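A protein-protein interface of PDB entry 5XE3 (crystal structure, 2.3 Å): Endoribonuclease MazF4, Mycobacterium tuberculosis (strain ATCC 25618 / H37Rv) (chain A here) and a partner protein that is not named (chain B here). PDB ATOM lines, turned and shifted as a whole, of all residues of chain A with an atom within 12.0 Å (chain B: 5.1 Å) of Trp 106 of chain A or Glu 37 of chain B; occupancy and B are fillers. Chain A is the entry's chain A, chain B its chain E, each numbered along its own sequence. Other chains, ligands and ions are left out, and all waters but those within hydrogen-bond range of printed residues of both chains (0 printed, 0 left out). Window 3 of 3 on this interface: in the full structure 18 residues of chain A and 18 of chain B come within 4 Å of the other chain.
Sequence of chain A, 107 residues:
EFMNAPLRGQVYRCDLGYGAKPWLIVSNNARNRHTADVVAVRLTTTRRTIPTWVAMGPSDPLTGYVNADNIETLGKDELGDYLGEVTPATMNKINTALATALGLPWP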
ATOM      1  N   ILE A  50      10.905  14.678 -22.221  1.00  0.00           N
ATOM      2  CA  ILE A  50      11.603  15.884 -22.691  1.00  0.00           C
ATOM      3  C   ILE A  50      10.463  16.866 -23.017  1.00  0.00           C
ATOM      4  O   ILE A  50       9.354  16.450 -23.400  1.00  0.00           O
ATOM      5  CB  ILE A  50      12.588  15.552 -23.869  1.00  0.00           C
ATOM      6  CG1 ILE A  50      13.331  16.780 -24.403  1.00  0.00           C
ATOM      7  CG2 ILE A  50      11.882  14.880 -25.034  1.00  0.00           C
ATOM      8  CD1 ILE A  50      14.491  16.443 -25.328  1.00  0.00           C
ATOM      9  N   PRO A  51      10.671  18.163 -22.792  1.00  0.00           N
ATOM     10  CA  PRO A  51       9.551  19.074 -23.084  1.00  0.00           C
ATOM     11  C   PRO A  51       9.032  19.093 -24.544  1.00  0.00           C
ATOM     12  O   PRO A  51       7.889  19.438 -24.754  1.00  0.00           O
ATOM     13  CB  PRO A  51      10.121  20.445 -22.696  1.00  0.00           C
ATOM     14  CG  PRO A  51      11.085  20.129 -21.625  1.00  0.00           C
ATOM     15  CD  PRO A  51      11.745  18.849 -22.067  1.00  0.00           C
ATOM     16  N   THR A  52       9.869  18.719 -25.513  1.00  0.00           N
ATOM     17  CA  THR A  52       9.456  18.608 -26.922  1.00  0.00           C
ATOM     18  C   THR A  52       8.591  17.393 -27.287  1.00  0.00           C
ATOM     19  O   THR A  52       8.146  17.268 -28.431  1.00  0.00           O
ATOM     20  CB  THR A  52      10.659  18.634 -27.836  1.00  0.00           C
ATOM     21  OG1 THR A  52      11.657  17.738 -27.341  1.00  0.00           O
ATOM     22  CG2 THR A  52      11.255  20.034 -27.880  1.00  0.00           C
ATOM     23  N   LYS A  93      -0.809  21.499 -26.324  1.00  0.00           N
ATOM     24  CA  LYS A  93       0.455  21.050 -25.761  1.00  0.00           C
ATOM     25  C   LYS A  93       1.546  20.908 -26.841  1.00  0.00           C
ATOM     26  O   LYS A  93       2.724  21.069 -26.574  1.00  0.00           O
ATOM     27  CB  LYS A  93       0.286  19.742 -25.016  1.00  0.00           C
ATOM     28  CG  LYS A  93      -0.486  19.876 -23.723  1.00  0.00           C
ATOM     29  CD  LYS A  93      -0.427  18.574 -22.907  1.00  0.00           C
ATOM     30  CE  LYS A  93      -1.637  18.422 -21.976  1.00  0.00           C
ATOM     31  NZ  LYS A  93      -2.919  18.154 -22.700  1.00  0.00           N
ATOM     32  N   ASN A  95       1.630  22.713 -29.615  1.00  0.00           N
ATOM     33  CA  ASN A  95       2.012  24.110 -29.873  1.00  0.00           C
ATOM     34  C   ASN A  95       3.195  24.544 -29.010  1.00  0.00           C
ATOM     35  O   ASN A  95       4.235  24.906 -29.520  1.00  0.00           O
ATOM     36  CB  ASN A  95       0.811  25.025 -29.669  1.00  0.00           C
ATOM     37  CG  ASN A  95      -0.270  24.781 -30.699  1.00  0.00           C
ATOM     38  OD1 ASN A  95      -0.015  24.183 -31.737  1.00  0.00           O
ATOM     39  ND2 ASN A  95      -1.489  25.219 -30.410  1.00  0.00           N
ATOM     40  N   THR A  96       3.035  24.421 -27.715  1.00  0.00           N
ATOM     41  CA  THR A  96       4.124  24.617 -26.761  1.00  0.00           C
ATOM     42  C   THR A  96       5.394  23.867 -27.094  1.00  0.00           C
ATOM     43  O   THR A  96       6.492  24.455 -27.056  1.00  0.00           O
ATOM     44  CB  THR A  96       3.666  24.187 -25.367  1.00  0.00           C
ATOM     45  OG1 THR A  96       2.639  25.070 -24.977  1.00  0.00           O
ATOM     46  CG2 THR A  96       4.773  24.288 -24.330  1.00  0.00           C
ATOM     47  N   ALA A  97       5.271  22.568 -27.369  1.00  0.00           N
ATOM     48  CA  ALA A  97       6.450  21.771 -27.662  1.00  0.00           C
ATOM     49  C   ALA A  97       7.161  22.219 -28.937  1.00  0.00           C
ATOM     50  O   ALA A  97       8.360  22.173 -29.022  1.00  0.00           O
ATOM     51  CB  ALA A  97       6.075  20.296 -27.761  1.00  0.00           C
ATOM     52  N   LEU A  98       6.398  22.549 -29.953  1.00  0.00           N
ATOM     53  CA  LEU A  98       6.924  23.064 -31.190  1.00  0.00           C
ATOM     54  C   LEU A  98       7.634  24.388 -30.978  1.00  0.00           C
ATOM     55  O   LEU A  98       8.711  24.605 -31.501  1.00  0.00           O
ATOM     56  CB  LEU A  98       5.796  23.312 -32.180  1.00  0.00           C
ATOM     57  CG  LEU A  98       5.618  22.308 -33.291  1.00  0.00           C
ATOM     58  CD1 LEU A  98       4.306  22.629 -34.018  1.00  0.00           C
ATOM     59  CD2 LEU A  98       6.826  22.373 -34.216  1.00  0.00           C
ATOM     60  N   ALA A  99       7.005  25.280 -30.234  1.00  0.00           N
ATOM     61  CA  ALA A  99       7.596  26.560 -29.983  1.00  0.00           C
ATOM     62  C   ALA A  99       8.927  26.341 -29.262  1.00  0.00           C
ATOM     63  O   ALA A  99       9.928  26.985 -29.580  1.00  0.00           O
ATOM     64  CB  ALA A  99       6.646  27.440 -29.165  1.00  0.00           C
ATOM     65  N   THR A 100       8.950  25.417 -28.312  1.00  0.00           N
ATOM     66  CA  THR A 100      10.186  25.085 -27.633  1.00  0.00           C
ATOM     67  C   THR A 100      11.232  24.543 -28.594  1.00  0.00           C
ATOM     68  O   THR A 100      12.394  24.942 -28.531  1.00  0.00           O
ATOM     69  CB  THR A 100       9.910  24.071 -26.533  1.00  0.00           C
ATOM     70  OG1 THR A 100       9.139  24.735 -25.545  1.00  0.00           O
ATOM     71  CG2 THR A 100      11.175  23.552 -25.912  1.00  0.00           C
ATOM     72  N   ALA A 101      10.822  23.651 -29.481  1.00  0.00           N
ATOM     73  CA  ALA A 101      11.742  23.092 -30.472  1.00  0.00           C
ATOM     74  C   ALA A 101      12.372  24.140 -31.398  1.00  0.00           C
ATOM     75  O   ALA A 101      13.534  24.037 -31.743  1.00  0.00           O
ATOM     76  CB  ALA A 101      11.054  22.025 -31.306  1.00  0.00           C
ATOM     77  N   LEU A 102      11.608  25.137 -31.778  1.00  0.00           N
ATOM     78  CA  LEU A 102      12.112  26.156 -32.696  1.00  0.00           C
ATOM     79  C   LEU A 102      12.512  27.417 -31.966  1.00  0.00           C
ATOM     80  O   LEU A 102      12.529  28.484 -32.584  1.00  0.00           O
ATOM     81  CB  LEU A 102      11.062  26.468 -33.769  1.00  0.00           C
ATOM     82  CG  LEU A 102      10.826  25.257 -34.643  1.00  0.00           C
ATOM     83  CD1 LEU A 102       9.635  25.505 -35.497  1.00  0.00           C
ATOM     84  CD2 LEU A 102      12.048  24.895 -35.486  1.00  0.00           C
ATOM     85  N   GLY A 103      12.821  27.282 -30.666  1.00  0.00           N
ATOM     86  CA  GLY A 103      13.390  28.330 -29.838  1.00  0.00           C
ATOM     87  C   GLY A 103      12.636  29.633 -29.864  1.00  0.00           C
ATOM     88  O   GLY A 103      13.235  30.689 -29.955  1.00  0.00           O
ATOM     89  N   LEU A 104      11.320  29.575 -29.827  1.00  0.00           N
ATOM     90  CA  LEU A 104      10.544  30.789 -29.708  1.00  0.00           C
ATOM     91  C   LEU A 104      10.726  31.383 -28.304  1.00  0.00           C
ATOM     92  O   LEU A 104      10.741  30.639 -27.328  1.00  0.00           O
ATOM     93  CB  LEU A 104       9.083  30.557 -30.061  1.00  0.00           C
ATOM     94  CG  LEU A 104       8.912  30.175 -31.528  1.00  0.00           C
ATOM     95  CD1 LEU A 104       7.441  30.239 -31.849  1.00  0.00           C
ATOM     96  CD2 LEU A 104       9.681  31.073 -32.485  1.00  0.00           C
ATOM     97  N   PRO A 105      10.926  32.725 -28.228  1.00  0.00           N
ATOM     98  CA  PRO A 105      11.386  33.328 -26.975  1.00  0.00           C
ATOM     99  C   PRO A 105      10.325  33.351 -25.875  1.00  0.00           C
ATOM    100  O   PRO A 105       9.140  33.168 -26.125  1.00  0.00           O
ATOM    101  CB  PRO A 105      11.822  34.757 -27.397  1.00  0.00           C
ATOM    102  CG  PRO A 105      11.059  35.043 -28.656  1.00  0.00           C
ATOM    103  CD  PRO A 105      10.955  33.701 -29.350  1.00  0.00           C
ATOM    104  N   TRP A 106      10.804  33.520 -24.654  1.00  0.00           N
ATOM    105  CA  TRP A 106       9.966  33.686 -23.487  1.00  0.00           C
ATOM    106  C   TRP A 106       9.316  35.067 -23.606  1.00  0.00           C
ATOM    107  O   TRP A 106       9.949  35.966 -24.170  1.00  0.00           O
ATOM    108  CB  TRP A 106      10.828  33.627 -22.217  1.00  0.00           C
ATOM    109  CG  TRP A 106      11.501  32.314 -22.011  1.00  0.00           C
ATOM    110  CD1 TRP A 106      12.842  32.034 -22.141  1.00  0.00           C
ATOM    111  CD2 TRP A 106      10.863  31.082 -21.632  1.00  0.00           C
ATOM    112  NE1 TRP A 106      13.071  30.705 -21.850  1.00  0.00           N
ATOM    113  CE2 TRP A 106      11.879  30.099 -21.535  1.00  0.00           C
ATOM    114  CE3 TRP A 106       9.526  30.715 -21.359  1.00  0.00           C
ATOM    115  CZ2 TRP A 106      11.604  28.774 -21.182  1.00  0.00           C
ATOM    116  CZ3 TRP A 106       9.255  29.386 -20.996  1.00  0.00           C
ATOM    117  CH2 TRP A 106      10.293  28.434 -20.917  1.00  0.00           C
ATOM    118  N   PRO A 107       8.088  35.255 -23.069  1.00  0.00           N
ATOM    119  CA  PRO A 107       7.293  34.325 -22.266  1.00  0.00           C
ATOM    120  C   PRO A 107       6.614  33.218 -23.081  1.00  0.00           C
ATOM    121  O   PRO A 107       6.535  32.061 -22.633  1.00  0.00           O
ATOM    122  CB  PRO A 107       6.225  35.239 -21.610  1.00  0.00           C
ATOM    123  CG  PRO A 107       6.564  36.643 -21.993  1.00  0.00           C
ATOM    124  CD  PRO A 107       7.369  36.532 -23.254  1.00  0.00           C
ATOM    125  N   ILE B  32      11.220  36.163 -10.367  1.00  0.00           N
ATOM    126  CA  ILE B  32      10.773  34.787 -10.130  1.00  0.00           C
ATOM    127  C   ILE B  32      10.527  34.120 -11.472  1.00  0.00           C
ATOM    128  O   ILE B  32      11.002  33.022 -11.728  1.00  0.00           O
ATOM    129  CB  ILE B  32       9.508  34.682  -9.250  1.00  0.00           C
ATOM    130  CG1 ILE B  32       9.760  35.240  -7.852  1.00  0.00           C
ATOM    131  CG2 ILE B  32       9.060  33.224  -9.144  1.00  0.00           C
ATOM    132  CD1 ILE B  32       8.496  35.679  -7.156  1.00  0.00           C
ATOM    133  N   ASN B  33       9.792  34.802 -12.343  1.00  0.00           N
ATOM    134  CA  ASN B  33       9.528  34.250 -13.676  1.00  0.00           C
ATOM    135  C   ASN B  33      10.769  33.996 -14.506  1.00  0.00           C
ATOM    136  O   ASN B  33      10.861  32.973 -15.148  1.00  0.00           O
ATOM    137  CB  ASN B  33       8.566  35.143 -14.444  1.00  0.00           C
ATOM    138  CG  ASN B  33       7.139  34.907 -14.014  1.00  0.00           C
ATOM    139  OD1 ASN B  33       6.638  33.792 -14.115  1.00  0.00           O
ATOM    140  ND2 ASN B  33       6.515  35.905 -13.475  1.00  0.00           N
ATOM    141  N   LYS B  34      11.731  34.903 -14.454  1.00  0.00           N
ATOM    142  CA  LYS B  34      12.978  34.697 -15.158  1.00  0.00           C
ATOM    143  C   LYS B  34      13.821  33.560 -14.579  1.00  0.00           C
ATOM    144  O   LYS B  34      14.424  32.811 -15.326  1.00  0.00           O
ATOM    145  CB  LYS B  34      13.776  36.008 -15.251  1.00  0.00           C
ATOM    146  CG  LYS B  34      13.351  36.760 -16.511  1.00  0.00           C
ATOM    147  CD  LYS B  34      13.859  38.175 -16.558  1.00  0.00           C
ATOM    148  CE  LYS B  34      13.834  38.751 -17.973  1.00  0.00           C
ATOM    149  NZ  LYS B  34      12.528  38.492 -18.586  1.00  0.00           N
ATOM    150  N   ARG B  35      13.832  33.413 -13.262  1.00  0.00           N
ATOM    151  CA  ARG B  35      14.509  32.294 -12.649  1.00  0.00           C
ATOM    152  C   ARG B  35      13.896  30.984 -13.110  1.00  0.00           C
ATOM    153  O   ARG B  35      14.634  30.013 -13.475  1.00  0.00           O
ATOM    154  CB  ARG B  35      14.484  32.394 -11.121  1.00  0.00           C
ATOM    155  CG  ARG B  35      15.234  31.295 -10.383  1.00  0.00           C
ATOM    156  CD  ARG B  35      16.735  31.283 -10.677  1.00  0.00           C
ATOM    157  NE  ARG B  35      17.336  30.065 -10.109  1.00  0.00           N
ATOM    158  CZ  ARG B  35      18.437  29.456 -10.545  1.00  0.00           C
ATOM    159  NH1 ARG B  35      19.127  29.916 -11.592  1.00  0.00           N
ATOM    160  NH2 ARG B  35      18.858  28.360  -9.909  1.00  0.00           N
ATOM    161  N   TRP B  36      12.559  30.944 -13.143  1.00  0.00           N
ATOM    162  CA  TRP B  36      11.879  29.710 -13.577  1.00  0.00           C
ATOM    163  C   TRP B  36      12.259  29.386 -15.017  1.00  0.00           C
ATOM    164  O   TRP B  36      12.584  28.222 -15.360  1.00  0.00           O
ATOM    165  CB  TRP B  36      10.363  29.840 -13.423  1.00  0.00           C
ATOM    166  CG  TRP B  36       9.609  28.600 -13.726  1.00  0.00           C
ATOM    167  CD1 TRP B  36       9.247  27.607 -12.846  1.00  0.00           C
ATOM    168  CD2 TRP B  36       9.075  28.228 -14.991  1.00  0.00           C
ATOM    169  NE1 TRP B  36       8.528  26.626 -13.501  1.00  0.00           N
ATOM    170  CE2 TRP B  36       8.408  26.979 -14.819  1.00  0.00           C
ATOM    171  CE3 TRP B  36       9.111  28.810 -16.261  1.00  0.00           C
ATOM    172  CZ2 TRP B  36       7.790  26.305 -15.874  1.00  0.00           C
ATOM    173  CZ3 TRP B  36       8.492  28.134 -17.320  1.00  0.00           C
ATOM    174  CH2 TRP B  36       7.847  26.891 -17.115  1.00  0.00           C
ATOM    175  N   GLU B  37      12.281  30.430 -15.849  1.00  0.00           N
ATOM    176  CA  GLU B  37      12.598  30.248 -17.268  1.00  0.00           C
ATOM    177  C   GLU B  37      14.011  29.747 -17.410  1.00  0.00           C
ATOM    178  O   GLU B  37      14.280  28.829 -18.171  1.00  0.00           O
ATOM    179  CB  GLU B  37      12.366  31.546 -18.081  1.00  0.00           C
ATOM    180  CG  GLU B  37      10.880  31.891 -18.171  1.00  0.00           C
ATOM    181  CD  GLU B  37      10.569  33.340 -18.548  1.00  0.00           C
ATOM    182  OE1 GLU B  37      11.493  34.112 -18.923  1.00  0.00           O
ATOM    183  OE2 GLU B  37       9.370  33.688 -18.474  1.00  0.00           O
ATOM    184  N   ALA B  38      14.915  30.346 -16.648  1.00  0.00           N
ATOM    185  CA  ALA B  38      16.298  29.906 -16.642  1.00  0.00           C
ATOM    186  C   ALA B  38      16.376  28.424 -16.217  1.00  0.00           C
ATOM    187  O   ALA B  38      17.046  27.643 -16.871  1.00  0.00           O
ATOM    188  CB  ALA B  38      17.139  30.806 -15.730  1.00  0.00           C
ATOM    189  N   LEU B  39      15.664  28.017 -15.173  1.00  0.00           N
ATOM    190  CA  LEU B  39      15.720  26.585 -14.764  1.00  0.00           C
ATOM    191  C   LEU B  39      15.048  25.662 -15.778  1.00  0.00           C
ATOM    192  O   LEU B  39      15.452  24.534 -15.940  1.00  0.00           O
ATOM    193  CB  LEU B  39      15.147  26.368 -13.356  1.00  0.00           C
ATOM    194  CG  LEU B  39      16.064  26.938 -12.249  1.00  0.00           C
ATOM    195  CD1 LEU B  39      15.299  27.249 -10.946  1.00  0.00           C
ATOM    196  CD2 LEU B  39      17.282  26.028 -12.009  1.00  0.00           C
ATOM    197  N   HIS B  40      14.020  26.148 -16.454  1.00  0.00           N
ATOM    198  CA  HIS B  40      13.406  25.380 -17.544  1.00  0.00           C
ATOM    199  C   HIS B  40      14.394  25.147 -18.714  1.00  0.00           C
ATOM    200  O   HIS B  40      14.438  24.050 -19.278  1.00  0.00           O
ATOM    201  CB  HIS B  40      12.109  26.064 -18.002  1.00  0.00           C
ATOM    202  CG  HIS B  40      11.257  25.232 -18.908  1.00  0.00           C
ATOM    203  ND1 HIS B  40      10.038  24.720 -18.519  1.00  0.00           N
ATOM    204  CD2 HIS B  40      11.430  24.852 -20.202  1.00  0.00           C
ATOM    205  CE1 HIS B  40       9.504  24.046 -19.526  1.00  0.00           C
ATOM    206  NE2 HIS B  40      10.329  24.107 -20.558  1.00  0.00           N
ATOM    207  N   ASP B  41      15.205  26.145 -19.060  1.00  0.00           N
ATOM    208  CA  ASP B  41      16.213  25.936 -20.098  1.00  0.00           C
ATOM    209  C   ASP B  41      17.354  24.963 -19.670  1.00  0.00           C
ATOM    210  O   ASP B  41      17.899  24.231 -20.514  1.00  0.00           O
ATOM    211  CB  ASP B  41      16.750  27.281 -20.592  1.00  0.00           C
ATOM    212  CG  ASP B  41      15.622  28.195 -21.239  1.00  0.00           C
ATOM    213  OD1 ASP B  41      14.674  27.653 -21.863  1.00  0.00           O
ATOM    214  OD2 ASP B  41      15.685  29.460 -21.108  1.00  0.00           O
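Hydrophobic or aromatic side chains of chain A that line the printed part of chain B: Trp 106.
Of the 10 printed residues of chain B, 4 touch a printed residue of chain A.
Hydrophobic or aromatic side chains of chain B that line the printed part of chain A: Trp 36 and His 40.
Among the printed residues, no Asp or Glu carboxylate lies within 4 Å of a Lys or Arg side-chain nitrogen of the other chain.
The indole nitrogen of Trp 106 of chain A is in hydrogen-bond range of the side-chain carboxylate of Asp 41 of chain B (3.0 Å).
CZ3 of Trp 36 of chain B touches CZ3 of Trp 106 of chain A, 3.96 Å away.
CB of Trp 106 of chain A touches OE1 of Glu 37 of chain B, 3.4 Å away.
CH2 of Trp 106 of chain A touches CD2 of His 40 of chain B, at 3.8 Å.
Asn 95 of chain A touches none of the printed residues of chain B.
Pro 105 of chain A touches none of the printed residues of chain B.
Trp 106 of chain A touches just these residues of chain B: Trp 36, Glu 37, His 40 and Asp 41.
No residue of chain A comes within 4 Å of Lys 34 of chain B.
Trp 36 of chain B touches just one residue of chain A: Trp 106 (3.96 Å).
Glu 37 of chain B touches one residue of chain A.
No residue of chain A comes within 4 Å of Ala 38 of chain B.
Asp 41 of chain B touches just one residue of chain A: Trp 106 (3.0 Å).
The nearest printed residue of chain B that does not touch Trp 106 of chain A is Ala 38 of chain B (5.5 Å).
The nearest residue of chain A that does not touch Glu 37 of chain B is Pro 107 of chain A (4.4 Å).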
